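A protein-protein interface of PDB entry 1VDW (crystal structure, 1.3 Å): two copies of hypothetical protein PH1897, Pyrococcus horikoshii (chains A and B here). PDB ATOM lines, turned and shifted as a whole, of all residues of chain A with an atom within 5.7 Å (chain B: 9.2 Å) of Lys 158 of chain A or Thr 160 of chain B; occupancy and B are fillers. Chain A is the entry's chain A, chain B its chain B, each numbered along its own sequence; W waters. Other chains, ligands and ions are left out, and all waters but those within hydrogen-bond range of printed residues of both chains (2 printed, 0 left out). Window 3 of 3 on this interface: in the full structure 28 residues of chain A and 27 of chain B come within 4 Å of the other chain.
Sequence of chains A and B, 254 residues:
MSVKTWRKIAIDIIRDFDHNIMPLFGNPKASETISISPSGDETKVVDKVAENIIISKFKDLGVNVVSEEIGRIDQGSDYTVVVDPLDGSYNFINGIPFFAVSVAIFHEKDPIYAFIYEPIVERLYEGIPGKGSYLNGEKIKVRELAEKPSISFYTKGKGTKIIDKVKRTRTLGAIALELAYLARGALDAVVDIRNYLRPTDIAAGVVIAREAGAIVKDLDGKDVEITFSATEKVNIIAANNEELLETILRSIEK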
ATOM      1  N   PHE A 153       9.766  -1.219  17.512  1.00  0.00           N
ATOM      2  CA  PHE A 153      10.193  -1.307  18.903  1.00  0.00           C
ATOM      3  C   PHE A 153       9.032  -1.302  19.884  1.00  0.00           C
ATOM      4  O   PHE A 153       8.184  -0.408  19.850  1.00  0.00           O
ATOM      5  CB  PHE A 153      11.149  -0.131  19.186  1.00  0.00           C
ATOM      6  CG  PHE A 153      11.758  -0.127  20.569  1.00  0.00           C
ATOM      7  CD1 PHE A 153      12.171  -1.306  21.186  1.00  0.00           C
ATOM      8  CD2 PHE A 153      11.985   1.083  21.222  1.00  0.00           C
ATOM      9  CE1 PHE A 153      12.805  -1.276  22.432  1.00  0.00           C
ATOM     10  CE2 PHE A 153      12.617   1.119  22.465  1.00  0.00           C
ATOM     11  CZ  PHE A 153      13.026  -0.062  23.067  1.00  0.00           C
ATOM     12  N   THR A 155       8.403  -1.983  24.137  1.00  0.00           N
ATOM     13  CA  THR A 155       8.983  -2.197  25.457  1.00  0.00           C
ATOM     14  C   THR A 155       8.056  -1.614  26.508  1.00  0.00           C
ATOM     15  O   THR A 155       7.253  -0.729  26.221  1.00  0.00           O
ATOM     16  CB  THR A 155      10.367  -1.537  25.600  1.00  0.00           C
ATOM     17  OG1 THR A 155      10.892  -1.828  26.904  1.00  0.00           O
ATOM     18  CG2 THR A 155      10.265  -0.031  25.424  1.00  0.00           C
ATOM     19  N   LYS A 156       8.163  -2.126  27.728  1.00  0.00           N
ATOM     20  CA  LYS A 156       7.349  -1.648  28.840  1.00  0.00           C
ATOM     21  C   LYS A 156       8.191  -0.693  29.673  1.00  0.00           C
ATOM     22  O   LYS A 156       7.673   0.033  30.523  1.00  0.00           O
ATOM     23  CB  LYS A 156       6.909  -2.825  29.715  1.00  0.00           C
ATOM     24  CG  LYS A 156       6.021  -3.847  29.017  1.00  0.00           C
ATOM     25  CD  LYS A 156       4.541  -3.501  29.141  1.00  0.00           C
ATOM     26  CE  LYS A 156       4.192  -2.185  28.465  1.00  0.00           C
ATOM     27  NZ  LYS A 156       2.754  -1.841  28.645  1.00  0.00           N
ATOM     28  N   GLY A 157       9.495  -0.693  29.420  1.00  0.00           N
ATOM     29  CA  GLY A 157      10.386   0.156  30.187  1.00  0.00           C
ATOM     30  C   GLY A 157      11.062   1.254  29.398  1.00  0.00           C
ATOM     31  O   GLY A 157      10.553   1.705  28.373  1.00  0.00           O
ATOM     32  N   LYS A 158      12.219   1.689  29.886  1.00  0.00           N
ATOM     33  CA  LYS A 158      12.971   2.750  29.235  1.00  0.00           C
ATOM     34  C   LYS A 158      13.639   2.244  27.965  1.00  0.00           C
ATOM     35  O   LYS A 158      14.189   1.143  27.930  1.00  0.00           O
ATOM     36  CB  LYS A 158      14.018   3.323  30.196  1.00  0.00           C
ATOM     37  CG  LYS A 158      14.877   4.426  29.590  1.00  0.00           C
ATOM     38  CD  LYS A 158      15.657   5.189  30.652  1.00  0.00           C
ATOM     39  CE  LYS A 158      14.733   6.044  31.508  1.00  0.00           C
ATOM     40  NZ  LYS A 158      15.490   6.879  32.485  1.00  0.00           N
ATOM     41  N   GLY A 159      13.577   3.052  26.914  1.00  0.00           N
ATOM     42  CA  GLY A 159      14.177   2.655  25.655  1.00  0.00           C
ATOM     43  C   GLY A 159      15.151   3.676  25.114  1.00  0.00           C
ATOM     44  O   GLY A 159      15.504   3.639  23.940  1.00  0.00           O
ATOM     45  N   THR A 160      15.595   4.584  25.977  1.00  0.00           N
ATOM     46  CA  THR A 160      16.527   5.633  25.585  1.00  0.00           C
ATOM     47  C   THR A 160      17.768   5.117  24.856  1.00  0.00           C
ATOM     48  O   THR A 160      18.126   5.623  23.791  1.00  0.00           O
ATOM     49  CB  THR A 160      16.984   6.438  26.817  1.00  0.00           C
ATOM     50  OG1 THR A 160      15.836   6.963  27.497  1.00  0.00           O
ATOM     51  CG2 THR A 160      17.893   7.588  26.399  1.00  0.00           C
ATOM     52  N   LYS A 161      18.424   4.112  25.429  1.00  0.00           N
ATOM     53  CA  LYS A 161      19.634   3.569  24.829  1.00  0.00           C
ATOM     54  C   LYS A 161      19.402   2.981  23.441  1.00  0.00           C
ATOM     55  O   LYS A 161      20.209   3.187  22.538  1.00  0.00           O
ATOM     56  CB  LYS A 161      20.265   2.524  25.754  1.00  0.00           C
ATOM     57  CG  LYS A 161      20.822   3.112  27.046  1.00  0.00           C
ATOM     58  CD  LYS A 161      21.440   2.035  27.922  1.00  0.00           C
ATOM     59  CE  LYS A 161      21.972   2.620  29.220  1.00  0.00           C
ATOM     60  NZ  LYS A 161      22.568   1.570  30.093  1.00  0.00           N
ATOM     61  N   ILE A 252      19.613  -2.927  25.929  1.00  0.00           N
ATOM     62  CA  ILE A 252      18.348  -3.193  26.601  1.00  0.00           C
ATOM     63  C   ILE A 252      18.353  -2.658  28.028  1.00  0.00           C
ATOM     64  O   ILE A 252      19.300  -2.875  28.786  1.00  0.00           O
ATOM     65  CB  ILE A 252      18.024  -4.706  26.612  1.00  0.00           C
ATOM     66  CG1 ILE A 252      17.735  -5.175  25.183  1.00  0.00           C
ATOM     67  CG2 ILE A 252      16.828  -4.981  27.516  1.00  0.00           C
ATOM     68  CD1 ILE A 252      17.368  -6.640  25.068  1.00  0.00           C
ATOM     69  N   GLU A 253      17.288  -1.944  28.377  1.00  0.00           N
ATOM     70  CA  GLU A 253      17.139  -1.359  29.704  1.00  0.00           C
ATOM     71  C   GLU A 253      15.884  -1.913  30.371  1.00  0.00           C
ATOM     72  O   GLU A 253      15.067  -2.569  29.723  1.00  0.00           O
ATOM     73  CB  GLU A 253      17.034   0.165  29.592  1.00  0.00           C
ATOM     74  CG  GLU A 253      18.288   0.843  29.059  1.00  0.00           C
ATOM     75  CD  GLU A 253      18.084   2.322  28.794  1.00  0.00           C
ATOM     76  OE1 GLU A 253      17.378   2.663  27.821  1.00  0.00           O
ATOM     77  OE2 GLU A 253      18.622   3.147  29.564  1.00  0.00           O
ATOM     78  N   LYS A 254      15.733  -1.649  31.665  1.00  0.00           N
ATOM     79  CA  LYS A 254      14.567  -2.128  32.398  1.00  0.00           C
ATOM     80  C   LYS A 254      13.417  -1.138  32.244  1.00  0.00           C
ATOM     81  O   LYS A 254      13.667  -0.031  31.725  1.00  0.00           O
ATOM     82  CB  LYS A 254      14.905  -2.295  33.883  1.00  0.00           C
ATOM     83  CG  LYS A 254      13.803  -2.963  34.695  1.00  0.00           C
ATOM     84  CD  LYS A 254      14.110  -2.951  36.185  1.00  0.00           C
ATOM     85  CE  LYS A 254      14.110  -1.535  36.740  1.00  0.00           C
ATOM     86  NZ  LYS A 254      14.347  -1.515  38.210  1.00  0.00           N
ATOM     87  OXT LYS A 254      12.285  -1.475  32.651  1.00  0.00           O
ATOM     88  N   ILE B 151      -2.621   5.448  22.798  1.00  0.00           N
ATOM     89  CA  ILE B 151      -2.013   6.685  22.323  1.00  0.00           C
ATOM     90  C   ILE B 151      -0.909   6.508  21.289  1.00  0.00           C
ATOM     91  O   ILE B 151      -0.321   5.435  21.153  1.00  0.00           O
ATOM     92  CB  ILE B 151      -1.382   7.489  23.506  1.00  0.00           C
ATOM     93  CG1 ILE B 151      -0.113   6.789  24.009  1.00  0.00           C
ATOM     94  CG2 ILE B 151      -2.379   7.618  24.654  1.00  0.00           C
ATOM     95  CD1 ILE B 151       0.679   7.606  25.030  1.00  0.00           C
ATOM     96  N   PHE B 153       2.751   7.691  20.415  1.00  0.00           N
ATOM     97  CA  PHE B 153       3.815   8.151  21.292  1.00  0.00           C
ATOM     98  C   PHE B 153       5.160   8.244  20.594  1.00  0.00           C
ATOM     99  O   PHE B 153       5.673   7.257  20.061  1.00  0.00           O
ATOM    100  CB  PHE B 153       3.876   7.181  22.484  1.00  0.00           C
ATOM    101  CG  PHE B 153       4.897   7.527  23.534  1.00  0.00           C
ATOM    102  CD1 PHE B 153       5.037   8.830  24.000  1.00  0.00           C
ATOM    103  CD2 PHE B 153       5.664   6.522  24.117  1.00  0.00           C
ATOM    104  CE1 PHE B 153       5.926   9.128  25.039  1.00  0.00           C
ATOM    105  CE2 PHE B 153       6.553   6.809  25.155  1.00  0.00           C
ATOM    106  CZ  PHE B 153       6.683   8.112  25.616  1.00  0.00           C
ATOM    107  N   THR B 155       9.056   9.665  21.255  1.00  0.00           N
ATOM    108  CA  THR B 155       9.974  10.099  22.284  1.00  0.00           C
ATOM    109  C   THR B 155      11.401   9.708  21.943  1.00  0.00           C
ATOM    110  O   THR B 155      11.634   8.822  21.121  1.00  0.00           O
ATOM    111  CB  THR B 155       9.585   9.468  23.632  1.00  0.00           C
ATOM    112  OG1 THR B 155      10.545   9.834  24.624  1.00  0.00           O
ATOM    113  CG2 THR B 155       9.524   7.946  23.517  1.00  0.00           C
ATOM    114  N   LYS B 156      12.352  10.390  22.568  1.00  0.00           N
ATOM    115  CA  LYS B 156      13.759  10.092  22.366  1.00  0.00           C
ATOM    116  C   LYS B 156      14.247   9.342  23.594  1.00  0.00           C
ATOM    117  O   LYS B 156      15.404   8.933  23.668  1.00  0.00           O
ATOM    118  CB  LYS B 156      14.558  11.383  22.172  1.00  0.00           C
ATOM    119  CG  LYS B 156      14.400  11.977  20.786  1.00  0.00           C
ATOM    120  CD  LYS B 156      15.037  11.074  19.741  1.00  0.00           C
ATOM    121  CE  LYS B 156      14.241  11.066  18.451  1.00  0.00           C
ATOM    122  NZ  LYS B 156      12.909  10.429  18.650  1.00  0.00           N
ATOM    123  N   GLY B 157      13.344   9.152  24.550  1.00  0.00           N
ATOM    124  CA  GLY B 157      13.693   8.442  25.767  1.00  0.00           C
ATOM    125  C   GLY B 157      12.862   8.849  26.970  1.00  0.00           C
ATOM    126  O   GLY B 157      12.699   8.074  27.910  1.00  0.00           O
ATOM    127  N   LYS B 158      12.339  10.070  26.950  1.00  0.00           N
ATOM    128  CA  LYS B 158      11.524  10.563  28.055  1.00  0.00           C
ATOM    129  C   LYS B 158      10.137   9.929  28.068  1.00  0.00           C
ATOM    130  O   LYS B 158       9.694   9.354  27.073  1.00  0.00           O
ATOM    131  CB  LYS B 158      11.363  12.083  27.964  1.00  0.00           C
ATOM    132  CG  LYS B 158      12.649  12.880  28.079  1.00  0.00           C
ATOM    133  CD  LYS B 158      12.353  14.372  28.044  1.00  0.00           C
ATOM    134  CE  LYS B 158      13.609  15.198  28.270  1.00  0.00           C
ATOM    135  NZ  LYS B 158      13.307  16.656  28.296  1.00  0.00           N
ATOM    136  N   GLY B 159       9.461  10.031  29.209  1.00  0.00           N
ATOM    137  CA  GLY B 159       8.111   9.515  29.326  1.00  0.00           C
ATOM    138  C   GLY B 159       7.870   8.050  29.642  1.00  0.00           C
ATOM    139  O   GLY B 159       6.791   7.542  29.352  1.00  0.00           O
ATOM    140  N   THR B 160       8.839   7.366  30.241  1.00  0.00           N
ATOM    141  CA  THR B 160       8.645   5.954  30.575  1.00  0.00           C
ATOM    142  C   THR B 160       7.414   5.764  31.464  1.00  0.00           C
ATOM    143  O   THR B 160       6.687   4.779  31.329  1.00  0.00           O
ATOM    144  CB  THR B 160       9.878   5.371  31.299  1.00  0.00           C
ATOM    145  OG1 THR B 160      11.012   5.423  30.427  1.00  0.00           O
ATOM    146  CG2 THR B 160       9.629   3.923  31.698  1.00  0.00           C
ATOM    147  N   LYS B 161       7.187   6.709  32.373  1.00  0.00           N
ATOM    148  CA  LYS B 161       6.045   6.652  33.282  1.00  0.00           C
ATOM    149  C   LYS B 161       4.704   6.718  32.554  1.00  0.00           C
ATOM    150  O   LYS B 161       3.660   6.418  33.129  1.00  0.00           O
ATOM    151  CB  LYS B 161       6.112   7.797  34.293  1.00  0.00           C
ATOM    152  CG  LYS B 161       7.154   7.648  35.382  1.00  0.00           C
ATOM    153  CD  LYS B 161       7.058   8.832  36.333  1.00  0.00           C
ATOM    154  CE  LYS B 161       7.983   8.691  37.525  1.00  0.00           C
ATOM    155  NZ  LYS B 161       7.835   9.852  38.450  1.00  0.00           N
ATOM    156  N   ILE B 162       4.727   7.129  31.292  1.00  0.00           N
ATOM    157  CA  ILE B 162       3.500   7.219  30.510  1.00  0.00           C
ATOM    158  C   ILE B 162       2.958   5.832  30.159  1.00  0.00           C
ATOM    159  O   ILE B 162       1.747   5.604  30.160  1.00  0.00           O
ATOM    160  CB  ILE B 162       3.739   7.990  29.188  1.00  0.00           C
ATOM    161  CG1 ILE B 162       4.092   9.448  29.491  1.00  0.00           C
ATOM    162  CG2 ILE B 162       2.496   7.911  28.299  1.00  0.00           C
ATOM    163  CD1 ILE B 162       4.494  10.242  28.258  1.00  0.00           C
ATOM    164  N   ILE B 163       3.872   4.910  29.878  1.00  0.00           N
ATOM    165  CA  ILE B 163       3.508   3.557  29.477  1.00  0.00           C
ATOM    166  C   ILE B 163       2.535   2.836  30.409  1.00  0.00           C
ATOM    167  O   ILE B 163       1.576   2.221  29.948  1.00  0.00           O
ATOM    168  CB  ILE B 163       4.780   2.695  29.276  1.00  0.00           C
ATOM    169  CG1 ILE B 163       5.753   3.413  28.338  1.00  0.00           C
ATOM    170  CG2 ILE B 163       4.407   1.340  28.689  1.00  0.00           C
ATOM    171  CD1 ILE B 163       5.158   3.780  26.995  1.00  0.00           C
ATOM    172  N   ASP B 164       2.761   2.918  31.716  1.00  0.00           N
ATOM    173  CA  ASP B 164       1.875   2.241  32.659  1.00  0.00           C
ATOM    174  C   ASP B 164       0.527   2.953  32.804  1.00  0.00           C
ATOM    175  O   ASP B 164      -0.391   2.430  33.435  1.00  0.00           O
ATOM    176  CB  ASP B 164       2.551   2.123  34.027  1.00  0.00           C
ATOM    177  CG  ASP B 164       2.671   3.454  34.732  1.00  0.00           C
ATOM    178  OD1 ASP B 164       1.680   3.890  35.356  1.00  0.00           O
ATOM    179  OD2 ASP B 164       3.754   4.069  34.651  1.00  0.00           O
ATOM    180  N   LYS B 165       0.405   4.138  32.209  1.00  0.00           N
ATOM    181  CA  LYS B 165      -0.835   4.907  32.284  1.00  0.00           C
ATOM    182  C   LYS B 165      -1.771   4.569  31.130  1.00  0.00           C
ATOM    183  O   LYS B 165      -2.937   4.971  31.123  1.00  0.00           O
ATOM    184  CB  LYS B 165      -0.540   6.409  32.236  1.00  0.00           C
ATOM    185  CG  LYS B 165       0.485   6.899  33.242  1.00  0.00           C
ATOM    186  CD  LYS B 165       0.017   6.689  34.672  1.00  0.00           C
ATOM    187  CE  LYS B 165       1.049   7.207  35.659  1.00  0.00           C
ATOM    188  NZ  LYS B 165       2.320   6.435  35.591  1.00  0.00           N
ATOM    189  N   VAL B 166      -1.260   3.835  30.151  1.00  0.00           N
ATOM    190  CA  VAL B 166      -2.059   3.485  28.985  1.00  0.00           C
ATOM    191  C   VAL B 166      -2.053   1.992  28.694  1.00  0.00           C
ATOM    192  O   VAL B 166      -1.197   1.257  29.177  1.00  0.00           O
ATOM    193  CB  VAL B 166      -1.563   4.251  27.730  1.00  0.00           C
ATOM    194  CG1 VAL B 166      -1.574   5.748  28.007  1.00  0.00           C
ATOM    195  CG2 VAL B 166      -0.168   3.789  27.341  1.00  0.00           C
ATOM    196  N   THR B 169       0.455   1.694  22.984  1.00  0.00           N
ATOM    197  CA  THR B 169       0.998   2.835  22.259  1.00  0.00           C
ATOM    198  C   THR B 169       1.202   2.445  20.801  1.00  0.00           C
ATOM    199  O   THR B 169       1.338   1.261  20.460  1.00  0.00           O
ATOM    200  CB  THR B 169       2.367   3.324  22.806  1.00  0.00           C
ATOM    201  OG1 THR B 169       3.366   2.320  22.599  1.00  0.00           O
ATOM    202  CG2 THR B 169       2.262   3.662  24.290  1.00  0.00           C
ATOM    203  N   ILE B 193       7.322  14.142  22.339  1.00  0.00           N
ATOM    204  CA  ILE B 193       8.247  14.848  23.216  1.00  0.00           C
ATOM    205  C   ILE B 193       9.699  14.651  22.771  1.00  0.00           C
ATOM    206  O   ILE B 193      10.620  14.577  23.596  1.00  0.00           O
ATOM    207  CB  ILE B 193       8.053  14.388  24.682  1.00  0.00           C
ATOM    208  CG1 ILE B 193       8.260  12.872  24.805  1.00  0.00           C
ATOM    209  CG2 ILE B 193       6.655  14.761  25.146  1.00  0.00           C
ATOM    210  CD1 ILE B 193       7.995  12.324  26.204  1.00  0.00           C
ATOM    211  N   ILE B 248      -0.354  12.561  31.717  1.00  0.00           N
ATOM    212  CA  ILE B 248       0.766  12.358  30.809  1.00  0.00           C
ATOM    213  C   ILE B 248       1.813  13.435  31.082  1.00  0.00           C
ATOM    214  O   ILE B 248       3.008  13.157  31.152  1.00  0.00           O
ATOM    215  CB  ILE B 248       0.305  12.448  29.343  1.00  0.00           C
ATOM    216  CG1 ILE B 248      -0.530  11.214  28.997  1.00  0.00           C
ATOM    217  CG2 ILE B 248       1.510  12.586  28.421  1.00  0.00           C
ATOM    218  CD1 ILE B 248      -1.178  11.278  27.626  1.00  0.00           C
ATOM    219  N   SER B 251       3.831  12.882  34.013  1.00  0.00           N
ATOM    220  CA  SER B 251       4.656  11.691  33.815  1.00  0.00           C
ATOM    221  C   SER B 251       5.860  11.907  32.896  1.00  0.00           C
ATOM    222  O   SER B 251       6.533  10.947  32.513  1.00  0.00           O
ATOM    223  CB  SER B 251       3.795  10.548  33.260  1.00  0.00           C
ATOM    224  OG  SER B 251       2.688  10.269  34.102  1.00  0.00           O
ATOM    225  N   ILE B 252       6.124  13.158  32.532  1.00  0.00           N
ATOM    226  CA  ILE B 252       7.248  13.480  31.656  1.00  0.00           C
ATOM    227  C   ILE B 252       8.330  14.249  32.411  1.00  0.00           C
ATOM    228  O   ILE B 252       8.035  15.226  33.100  1.00  0.00           O
ATOM    229  CB  ILE B 252       6.771  14.326  30.456  1.00  0.00           C
ATOM    230  CG1 ILE B 252       5.815  13.498  29.596  1.00  0.00           C
ATOM    231  CG2 ILE B 252       7.963  14.793  29.632  1.00  0.00           C
ATOM    232  CD1 ILE B 252       5.140  14.288  28.496  1.00  0.00           C
ATOM    233  N   GLU B 253       9.580  13.813  32.271  1.00  0.00           N
ATOM    234  CA  GLU B 253      10.702  14.467  32.948  1.00  0.00           C
ATOM    235  C   GLU B 253      11.087  15.773  32.263  1.00  0.00           C
ATOM    236  O   GLU B 253      10.752  15.999  31.101  1.00  0.00           O
ATOM    237  CB  GLU B 253      11.937  13.559  32.975  1.00  0.00           C
ATOM    238  CG  GLU B 253      11.681  12.099  33.286  1.00  0.00           C
ATOM    239  CD  GLU B 253      11.476  11.273  32.032  1.00  0.00           C
ATOM    240  OE1 GLU B 253      10.465  11.490  31.337  1.00  0.00           O
ATOM    241  OE2 GLU B 253      12.332  10.411  31.737  1.00  0.00           O
ATOM    242  N   LYS B 254      11.806  16.622  32.995  1.00  0.00           N
ATOM    243  CA  LYS B 254      12.272  17.911  32.488  1.00  0.00           C
ATOM    244  C   LYS B 254      11.149  18.786  31.942  1.00  0.00           C
ATOM    245  O   LYS B 254      10.890  19.847  32.551  1.00  0.00           O
ATOM    246  CB  LYS B 254      13.335  17.704  31.401  1.00  0.00           C
ATOM    247  CG  LYS B 254      14.622  17.045  31.887  1.00  0.00           C
ATOM    248  CD  LYS B 254      14.376  15.627  32.372  1.00  0.00           C
ATOM    249  CE  LYS B 254      15.633  15.002  32.945  1.00  0.00           C
ATOM    250  NZ  LYS B 254      15.368  13.646  33.503  1.00  0.00           N
ATOM    251  OXT LYS B 254      10.541  18.407  30.917  1.00  0.00           O
HETATM  252  O   HOH W   1      17.719   8.190  22.892  1.00  0.00           O
HETATM  253  O   HOH W   2       1.090   0.233  28.069  1.00  0.00           O
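CE of Lys 156 of chain A touches CG2 of Ile 163 of chain B, at 3.5 Å.
Gly 157 of chain A touches Thr 160 of chain B (C to CG2, 3.8 Å).
OG1 of Thr 160 of chain B touches CA of Lys 158 of chain A, at 3.5 Å.
Thr 160 of chain A touches Lys 156 of chain B (CG2 to O, 3.9 Å).
Gly 157 of chain A touches Thr 160 of chain B, and with the chains exchanged Thr 160 of chain A touches Gly 157 of chain B.
Lys 158 of chain A touches Thr 160 of chain B, but with the chains exchanged Thr 160 of chain A does not touch Lys 158 of chain B (4.7 Å).
Thr 160 of chain A touches Lys 156 of chain B, but with the chains exchanged Lys 156 of chain A does not touch Thr 160 of chain B (4.5 Å).
11 positions are printed for both chains.
Of the 5 pairs that touch across the chains among the printed residues, 2 have their exchanged pair printed and touching as well.
Of the 11 printed residues of chain A, 4 touch a printed residue of chain B.
Along chain B the printed residues that touch a printed residue of chain A span positions 156 to 163.
OG1 of Thr 160 of chain A sits close to O of Gly 157 of chain B, at 3.4 Å.
The backbone NH of Thr 160 of chain A sits at hydrogen-bond distance from the side-chain carboxylate of Glu 253 of chain A (3.2 Å).
The backbone NH (N) of Lys 158 of chain A lies within hydrogen-bond range of the chain-end carboxylate (O) of Lys 254 of chain A (2.9 Å).
N of Gly 157 of chain B lies within hydrogen-bond range of OG1 of Thr 155 of chain B.
N of Gly 157 of chain A sits at hydrogen-bond distance from OG1 of Thr 155 of chain A, 3.1 Å away.
Water W1 lies within hydrogen-bond range of the backbone carbonyl oxygen (O) of Lys 156 of chain B (2.6 Å) and the backbone carbonyl oxygen (O) of Thr 160 of chain A (2.8 Å).
Water W2 lies within hydrogen-bond range of the side-chain amino group of Lys 156 of chain A, the backbone carbonyl oxygen of Val 166 of chain B and the backbone carbonyl oxygen of Ile 163 of chain B.
Thr 155 of chain A touches none of the printed residues of chain B.
Of the printed residues of chain B, Lys 156 of chain A touches Ile 163 (3.5 Å).
Lys 158 of chain A touches one residue of chain B.
Ile 252 of chain A touches none of the printed residues of chain B.
No residue of chain B comes within 4 Å of Glu 253 of chain A.
Printed residues of chain A within 4 Å of Lys 156 of chain B: Thr 160 (3.9 Å).
Of the printed residues of chain A, Gly 157 of chain B touches Thr 160 (3.1 Å).
Of chain A, only Gly 157 (3.8 Å) and Lys 158 (3.5 Å) come within 4 Å of Thr 160 of chain B.
Of the printed residues of chain A, Ile 163 of chain B touches Lys 156.
The nearest printed residue of chain A that does not touch Ile 163 of chain B is Thr 155 of chain A (4.3 Å).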
